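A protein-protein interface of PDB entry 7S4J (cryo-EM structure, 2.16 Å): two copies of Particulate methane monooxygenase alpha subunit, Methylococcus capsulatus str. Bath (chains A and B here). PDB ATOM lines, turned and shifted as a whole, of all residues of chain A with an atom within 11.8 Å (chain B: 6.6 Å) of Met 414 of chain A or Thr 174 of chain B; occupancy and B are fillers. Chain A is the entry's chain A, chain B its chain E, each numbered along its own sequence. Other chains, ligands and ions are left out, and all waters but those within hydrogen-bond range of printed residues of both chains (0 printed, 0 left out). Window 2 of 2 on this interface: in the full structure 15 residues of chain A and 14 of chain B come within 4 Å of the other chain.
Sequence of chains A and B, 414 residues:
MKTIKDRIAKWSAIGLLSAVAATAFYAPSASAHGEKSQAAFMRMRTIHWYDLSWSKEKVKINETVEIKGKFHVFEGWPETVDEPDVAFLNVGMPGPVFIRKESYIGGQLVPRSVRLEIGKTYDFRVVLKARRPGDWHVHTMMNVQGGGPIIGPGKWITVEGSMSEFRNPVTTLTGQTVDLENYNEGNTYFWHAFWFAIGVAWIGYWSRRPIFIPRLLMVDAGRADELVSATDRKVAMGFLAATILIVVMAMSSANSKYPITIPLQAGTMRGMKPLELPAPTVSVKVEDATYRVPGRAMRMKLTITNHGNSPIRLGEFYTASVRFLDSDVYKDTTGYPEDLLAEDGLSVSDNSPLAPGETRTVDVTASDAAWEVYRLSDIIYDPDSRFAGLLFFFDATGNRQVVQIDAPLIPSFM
SD of Met 414 of chain A lies close to O of Leu 173 of chain B (3.4 Å).
O of Phe 413 of chain A lies within hydrogen-bond range of NH2 of Arg 292 of chain A, 3.0 Å away. The guanidinium group (NH1) of Arg 292 of chain A sits at hydrogen-bond distance from the backbone carbonyl oxygen (O) of Met 414 of chain A, 2.7 Å away. OG1 of Thr 172 of chain B lies within hydrogen-bond range of OG1 of Thr 174 of chain B (2.5 Å).
CD1 of Leu 173 of chain B touches O of Pro 411 of chain A, at 3.8 Å. Leu 173 of chain B touches Phe 413 of chain A (CB to CE2, 3.9 Å). CG2 of Ile 260 of chain B touches CZ of Phe 413 of chain A (3.4 Å). Met 414 of chain A touches Thr 174 of chain B. N of Gly 175 of chain B touches CE of Met 414 of chain A (3.6 Å).
Pro 294 of chain A touches none of the printed residues of chain B. Of the printed residues of chain B, Pro 411 of chain A touches Leu 173. Of the printed residues of chain B, Phe 413 of chain A touches Leu 173 (3.9 Å) and Ile 260 (3.4 Å). Thr 171 of chain B touches none of the printed residues of chain A. No residue of chain A comes within 4 Å of Thr 172 of chain B. Of chain A, only Met 414 comes within 4 Å of Thr 174 of chain B. Gly 175 of chain B touches just one residue of chain A: Met 414. No residue of chain A comes within 4 Å of Gln 176 of chain B. No residue of chain A comes within 4 Å of Pro 259 of chain B. The nearest printed residue of chain B that does not touch Pro 411 of chain A is Ile 260 of chain B (6.8 Å).
Hydrophobic or aromatic side chains of chain B within 4 Å of the printed part of chain A: Leu 173 and Ile 260. Of the 13 printed residues of chain A, 3 touch a printed residue of chain B. Hydrophobic or aromatic side chains of chain A that line the printed part of chain B: Phe 413 and Met 414. Among the printed residues, 6 pairs touch across the chains. Among the printed residues, no Asp or Glu carboxylate lies within 4 Å of a Lys or Arg side-chain nitrogen of the other chain.
No position is printed for both chains.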
ATOM      1  N   THR A 290     -12.515 -10.992  14.189  1.00  0.00           N
ATOM      2  CA  THR A 290     -13.971 -11.255  14.028  1.00  0.00           C
ATOM      3  C   THR A 290     -14.325 -12.731  14.235  1.00  0.00           C
ATOM      4  O   THR A 290     -13.408 -13.532  14.485  1.00  0.00           O
ATOM      5  CB  THR A 290     -14.479 -10.833  12.641  1.00  0.00           C
ATOM      6  OG1 THR A 290     -13.773 -11.576  11.647  1.00  0.00           O
ATOM      7  CG2 THR A 290     -14.347  -9.349  12.375  1.00  0.00           C
ATOM      8  N   TYR A 291     -15.617 -13.062  14.149  1.00  0.00           N
ATOM      9  CA  TYR A 291     -16.083 -14.474  14.244  1.00  0.00           C
ATOM     10  C   TYR A 291     -17.485 -14.539  13.630  1.00  0.00           C
ATOM     11  O   TYR A 291     -18.244 -13.562  13.752  1.00  0.00           O
ATOM     12  CB  TYR A 291     -16.019 -15.015  15.677  1.00  0.00           C
ATOM     13  CG  TYR A 291     -17.077 -14.489  16.608  1.00  0.00           C
ATOM     14  CD1 TYR A 291     -16.990 -13.208  17.119  1.00  0.00           C
ATOM     15  CD2 TYR A 291     -18.164 -15.267  16.972  1.00  0.00           C
ATOM     16  CE1 TYR A 291     -17.945 -12.710  17.984  1.00  0.00           C
ATOM     17  CE2 TYR A 291     -19.137 -14.780  17.827  1.00  0.00           C
ATOM     18  CZ  TYR A 291     -19.030 -13.494  18.322  1.00  0.00           C
ATOM     19  OH  TYR A 291     -19.969 -12.990  19.163  1.00  0.00           O
ATOM     20  N   ARG A 292     -17.825 -15.655  12.988  1.00  0.00           N
ATOM     21  CA  ARG A 292     -19.102 -15.760  12.302  1.00  0.00           C
ATOM     22  C   ARG A 292     -20.185 -16.245  13.255  1.00  0.00           C
ATOM     23  O   ARG A 292     -19.943 -17.099  14.111  1.00  0.00           O
ATOM     24  CB  ARG A 292     -18.991 -16.711  11.114  1.00  0.00           C
ATOM     25  CG  ARG A 292     -18.182 -16.163   9.956  1.00  0.00           C
ATOM     26  CD  ARG A 292     -19.085 -15.523   8.927  1.00  0.00           C
ATOM     27  NE  ARG A 292     -20.471 -15.930   9.115  1.00  0.00           N
ATOM     28  CZ  ARG A 292     -21.521 -15.185   8.797  1.00  0.00           C
ATOM     29  NH1 ARG A 292     -21.378 -13.986   8.257  1.00  0.00           N
ATOM     30  NH2 ARG A 292     -22.743 -15.656   9.023  1.00  0.00           N
ATOM     31  N   VAL A 293     -21.377 -15.680  13.111  1.00  0.00           N
ATOM     32  CA  VAL A 293     -22.541 -16.113  13.877  1.00  0.00           C
ATOM     33  C   VAL A 293     -23.622 -16.551  12.896  1.00  0.00           C
ATOM     34  O   VAL A 293     -24.173 -15.711  12.173  1.00  0.00           O
ATOM     35  CB  VAL A 293     -23.056 -14.999  14.802  1.00  0.00           C
ATOM     36  CG1 VAL A 293     -24.097 -15.545  15.756  1.00  0.00           C
ATOM     37  CG2 VAL A 293     -21.909 -14.370  15.567  1.00  0.00           C
ATOM     38  N   PRO A 294     -23.951 -17.849  12.821  1.00  0.00           N
ATOM     39  CA  PRO A 294     -23.324 -18.936  13.575  1.00  0.00           C
ATOM     40  C   PRO A 294     -22.041 -19.428  12.918  1.00  0.00           C
ATOM     41  O   PRO A 294     -21.800 -19.146  11.747  1.00  0.00           O
ATOM     42  CB  PRO A 294     -24.392 -20.038  13.569  1.00  0.00           C
ATOM     43  CG  PRO A 294     -25.508 -19.543  12.671  1.00  0.00           C
ATOM     44  CD  PRO A 294     -25.006 -18.353  11.932  1.00  0.00           C
ATOM     45  N   GLY A 295     -21.230 -20.157  13.670  1.00  0.00           N
ATOM     46  CA  GLY A 295     -20.005 -20.704  13.123  1.00  0.00           C
ATOM     47  C   GLY A 295     -19.198 -21.355  14.221  1.00  0.00           C
ATOM     48  O   GLY A 295     -19.522 -21.260  15.408  1.00  0.00           O
ATOM     49  N   ARG A 299     -11.627 -15.631  13.462  1.00  0.00           N
ATOM     50  CA  ARG A 299     -10.665 -15.118  12.501  1.00  0.00           C
ATOM     51  C   ARG A 299     -10.079 -13.811  13.009  1.00  0.00           C
ATOM     52  O   ARG A 299     -10.807 -12.938  13.488  1.00  0.00           O
ATOM     53  CB  ARG A 299     -11.322 -14.909  11.135  1.00  0.00           C
ATOM     54  CG  ARG A 299     -10.403 -14.346  10.079  1.00  0.00           C
ATOM     55  CD  ARG A 299     -11.077 -13.226   9.313  1.00  0.00           C
ATOM     56  NE  ARG A 299     -11.435 -12.118  10.189  1.00  0.00           N
ATOM     57  CZ  ARG A 299     -10.645 -11.086  10.452  1.00  0.00           C
ATOM     58  NH1 ARG A 299      -9.443 -10.979   9.910  1.00  0.00           N
ATOM     59  NH2 ARG A 299     -11.072 -10.138  11.280  1.00  0.00           N
ATOM     60  N   ILE A 380     -21.365 -13.749  22.035  1.00  0.00           N
ATOM     61  CA  ILE A 380     -22.328 -12.798  21.489  1.00  0.00           C
ATOM     62  C   ILE A 380     -23.379 -12.431  22.527  1.00  0.00           C
ATOM     63  O   ILE A 380     -24.033 -11.389  22.418  1.00  0.00           O
ATOM     64  CB  ILE A 380     -22.971 -13.365  20.211  1.00  0.00           C
ATOM     65  CG1 ILE A 380     -23.634 -12.244  19.414  1.00  0.00           C
ATOM     66  CG2 ILE A 380     -23.960 -14.468  20.546  1.00  0.00           C
ATOM     67  CD1 ILE A 380     -24.296 -12.712  18.164  1.00  0.00           C
ATOM     68  N   ILE A 410     -15.440  -8.996  17.114  1.00  0.00           N
ATOM     69  CA  ILE A 410     -16.596  -8.436  16.421  1.00  0.00           C
ATOM     70  C   ILE A 410     -17.352  -9.572  15.741  1.00  0.00           C
ATOM     71  O   ILE A 410     -16.785 -10.234  14.862  1.00  0.00           O
ATOM     72  CB  ILE A 410     -16.175  -7.372  15.398  1.00  0.00           C
ATOM     73  CG1 ILE A 410     -15.244  -6.346  16.046  1.00  0.00           C
ATOM     74  CG2 ILE A 410     -17.394  -6.696  14.810  1.00  0.00           C
ATOM     75  CD1 ILE A 410     -15.857  -5.605  17.205  1.00  0.00           C
ATOM     76  N   PRO A 411     -18.604  -9.828  16.104  1.00  0.00           N
ATOM     77  CA  PRO A 411     -19.390 -10.821  15.369  1.00  0.00           C
ATOM     78  C   PRO A 411     -19.692 -10.357  13.955  1.00  0.00           C
ATOM     79  O   PRO A 411     -19.815  -9.163  13.678  1.00  0.00           O
ATOM     80  CB  PRO A 411     -20.670 -10.941  16.198  1.00  0.00           C
ATOM     81  CG  PRO A 411     -20.785  -9.632  16.880  1.00  0.00           C
ATOM     82  CD  PRO A 411     -19.383  -9.200  17.181  1.00  0.00           C
ATOM     83  N   SER A 412     -19.805 -11.324  13.052  1.00  0.00           N
ATOM     84  CA  SER A 412     -20.207 -11.065  11.679  1.00  0.00           C
ATOM     85  C   SER A 412     -21.392 -11.957  11.351  1.00  0.00           C
ATOM     86  O   SER A 412     -21.351 -13.164  11.599  1.00  0.00           O
ATOM     87  CB  SER A 412     -19.056 -11.314  10.702  1.00  0.00           C
ATOM     88  OG  SER A 412     -18.743 -12.688  10.627  1.00  0.00           O
ATOM     89  N   PHE A 413     -22.442 -11.362  10.796  1.00  0.00           N
ATOM     90  CA  PHE A 413     -23.689 -12.070  10.538  1.00  0.00           C
ATOM     91  C   PHE A 413     -23.960 -12.260   9.057  1.00  0.00           C
ATOM     92  O   PHE A 413     -24.570 -13.263   8.668  1.00  0.00           O
ATOM     93  CB  PHE A 413     -24.858 -11.326  11.202  1.00  0.00           C
ATOM     94  CG  PHE A 413     -24.574 -10.894  12.610  1.00  0.00           C
ATOM     95  CD1 PHE A 413     -24.762 -11.768  13.662  1.00  0.00           C
ATOM     96  CD2 PHE A 413     -24.111  -9.621  12.881  1.00  0.00           C
ATOM     97  CE1 PHE A 413     -24.499 -11.381  14.954  1.00  0.00           C
ATOM     98  CE2 PHE A 413     -23.845  -9.229  14.175  1.00  0.00           C
ATOM     99  CZ  PHE A 413     -24.038 -10.111  15.212  1.00  0.00           C
ATOM    100  N   MET A 414     -23.529 -11.329   8.215  1.00  0.00           N
ATOM    101  CA  MET A 414     -23.739 -11.459   6.779  1.00  0.00           C
ATOM    102  C   MET A 414     -22.469 -11.954   6.096  1.00  0.00           C
ATOM    103  O   MET A 414     -21.366 -11.783   6.617  1.00  0.00           O
ATOM    104  CB  MET A 414     -24.180 -10.128   6.170  1.00  0.00           C
ATOM    105  CG  MET A 414     -23.444  -8.913   6.707  1.00  0.00           C
ATOM    106  SD  MET A 414     -24.510  -7.468   6.852  1.00  0.00           S
ATOM    107  CE  MET A 414     -23.308  -6.205   7.262  1.00  0.00           C
ATOM    108  N   THR B 171     -23.717   3.001  10.661  1.00  0.00           N
ATOM    109  CA  THR B 171     -23.972   1.758   9.950  1.00  0.00           C
ATOM    110  C   THR B 171     -23.862   0.585  10.913  1.00  0.00           C
ATOM    111  O   THR B 171     -22.846   0.428  11.595  1.00  0.00           O
ATOM    112  CB  THR B 171     -22.990   1.584   8.790  1.00  0.00           C
ATOM    113  OG1 THR B 171     -23.082   2.713   7.915  1.00  0.00           O
ATOM    114  CG2 THR B 171     -23.306   0.321   8.012  1.00  0.00           C
ATOM    115  N   THR B 172     -24.905  -0.232  10.966  1.00  0.00           N
ATOM    116  CA  THR B 172     -24.935  -1.377  11.858  1.00  0.00           C
ATOM    117  C   THR B 172     -24.281  -2.592  11.203  1.00  0.00           C
ATOM    118  O   THR B 172     -24.011  -2.618  10.003  1.00  0.00           O
ATOM    119  CB  THR B 172     -26.372  -1.704  12.259  1.00  0.00           C
ATOM    120  OG1 THR B 172     -27.031  -2.374  11.181  1.00  0.00           O
ATOM    121  CG2 THR B 172     -27.130  -0.435  12.597  1.00  0.00           C
ATOM    122  N   LEU B 173     -24.017  -3.610  12.023  1.00  0.00           N
ATOM    123  CA  LEU B 173     -23.498  -4.871  11.514  1.00  0.00           C
ATOM    124  C   LEU B 173     -24.551  -5.673  10.767  1.00  0.00           C
ATOM    125  O   LEU B 173     -24.208  -6.673  10.131  1.00  0.00           O
ATOM    126  CB  LEU B 173     -22.925  -5.706  12.657  1.00  0.00           C
ATOM    127  CG  LEU B 173     -21.598  -5.209  13.225  1.00  0.00           C
ATOM    128  CD1 LEU B 173     -21.344  -5.808  14.589  1.00  0.00           C
ATOM    129  CD2 LEU B 173     -20.466  -5.532  12.276  1.00  0.00           C
ATOM    130  N   THR B 174     -25.816  -5.265  10.836  1.00  0.00           N
ATOM    131  CA  THR B 174     -26.879  -5.902  10.074  1.00  0.00           C
ATOM    132  C   THR B 174     -27.039  -5.303   8.686  1.00  0.00           C
ATOM    133  O   THR B 174     -27.941  -5.714   7.952  1.00  0.00           O
ATOM    134  CB  THR B 174     -28.204  -5.795  10.826  1.00  0.00           C
ATOM    135  OG1 THR B 174     -28.407  -4.440  11.245  1.00  0.00           O
ATOM    136  CG2 THR B 174     -28.183  -6.685  12.052  1.00  0.00           C
ATOM    137  N   GLY B 175     -26.202  -4.337   8.318  1.00  0.00           N
ATOM    138  CA  GLY B 175     -26.253  -3.755   6.995  1.00  0.00           C
ATOM    139  C   GLY B 175     -27.221  -2.610   6.823  1.00  0.00           C
ATOM    140  O   GLY B 175     -27.659  -2.351   5.697  1.00  0.00           O
ATOM    141  N   GLN B 176     -27.566  -1.907   7.896  1.00  0.00           N
ATOM    142  CA  GLN B 176     -28.502  -0.796   7.811  1.00  0.00           C
ATOM    143  C   GLN B 176     -27.832   0.474   8.305  1.00  0.00           C
ATOM    144  O   GLN B 176     -27.095   0.454   9.292  1.00  0.00           O
ATOM    145  CB  GLN B 176     -29.773  -1.068   8.622  1.00  0.00           C
ATOM    146  CG  GLN B 176     -30.224  -2.514   8.598  1.00  0.00           C
ATOM    147  CD  GLN B 176     -31.234  -2.787   7.499  1.00  0.00           C
ATOM    148  OE1 GLN B 176     -32.080  -1.946   7.196  1.00  0.00           O
ATOM    149  NE2 GLN B 176     -31.147  -3.965   6.896  1.00  0.00           N
ATOM    150  N   PRO B 259     -33.776  -9.613  14.402  1.00  0.00           N
ATOM    151  CA  PRO B 259     -33.442 -10.931  14.956  1.00  0.00           C
ATOM    152  C   PRO B 259     -32.073 -10.981  15.607  1.00  0.00           C
ATOM    153  O   PRO B 259     -31.808 -11.913  16.373  1.00  0.00           O
ATOM    154  CB  PRO B 259     -33.513 -11.852  13.734  1.00  0.00           C
ATOM    155  CG  PRO B 259     -33.174 -10.970  12.596  1.00  0.00           C
ATOM    156  CD  PRO B 259     -33.684  -9.598  12.931  1.00  0.00           C
ATOM    157  N   ILE B 260     -31.201 -10.020  15.329  1.00  0.00           N
ATOM    158  CA  ILE B 260     -29.850  -9.990  15.873  1.00  0.00           C
ATOM    159  C   ILE B 260     -29.754  -8.805  16.822  1.00  0.00           C
ATOM    160  O   ILE B 260     -29.825  -7.648  16.393  1.00  0.00           O
ATOM    161  CB  ILE B 260     -28.792  -9.893  14.769  1.00  0.00           C
ATOM    162  CG1 ILE B 260     -28.739 -11.189  13.961  1.00  0.00           C
ATOM    163  CG2 ILE B 260     -27.439  -9.580  15.364  1.00  0.00           C
ATOM    164  CD1 ILE B 260     -28.959 -10.985  12.489  1.00  0.00           C
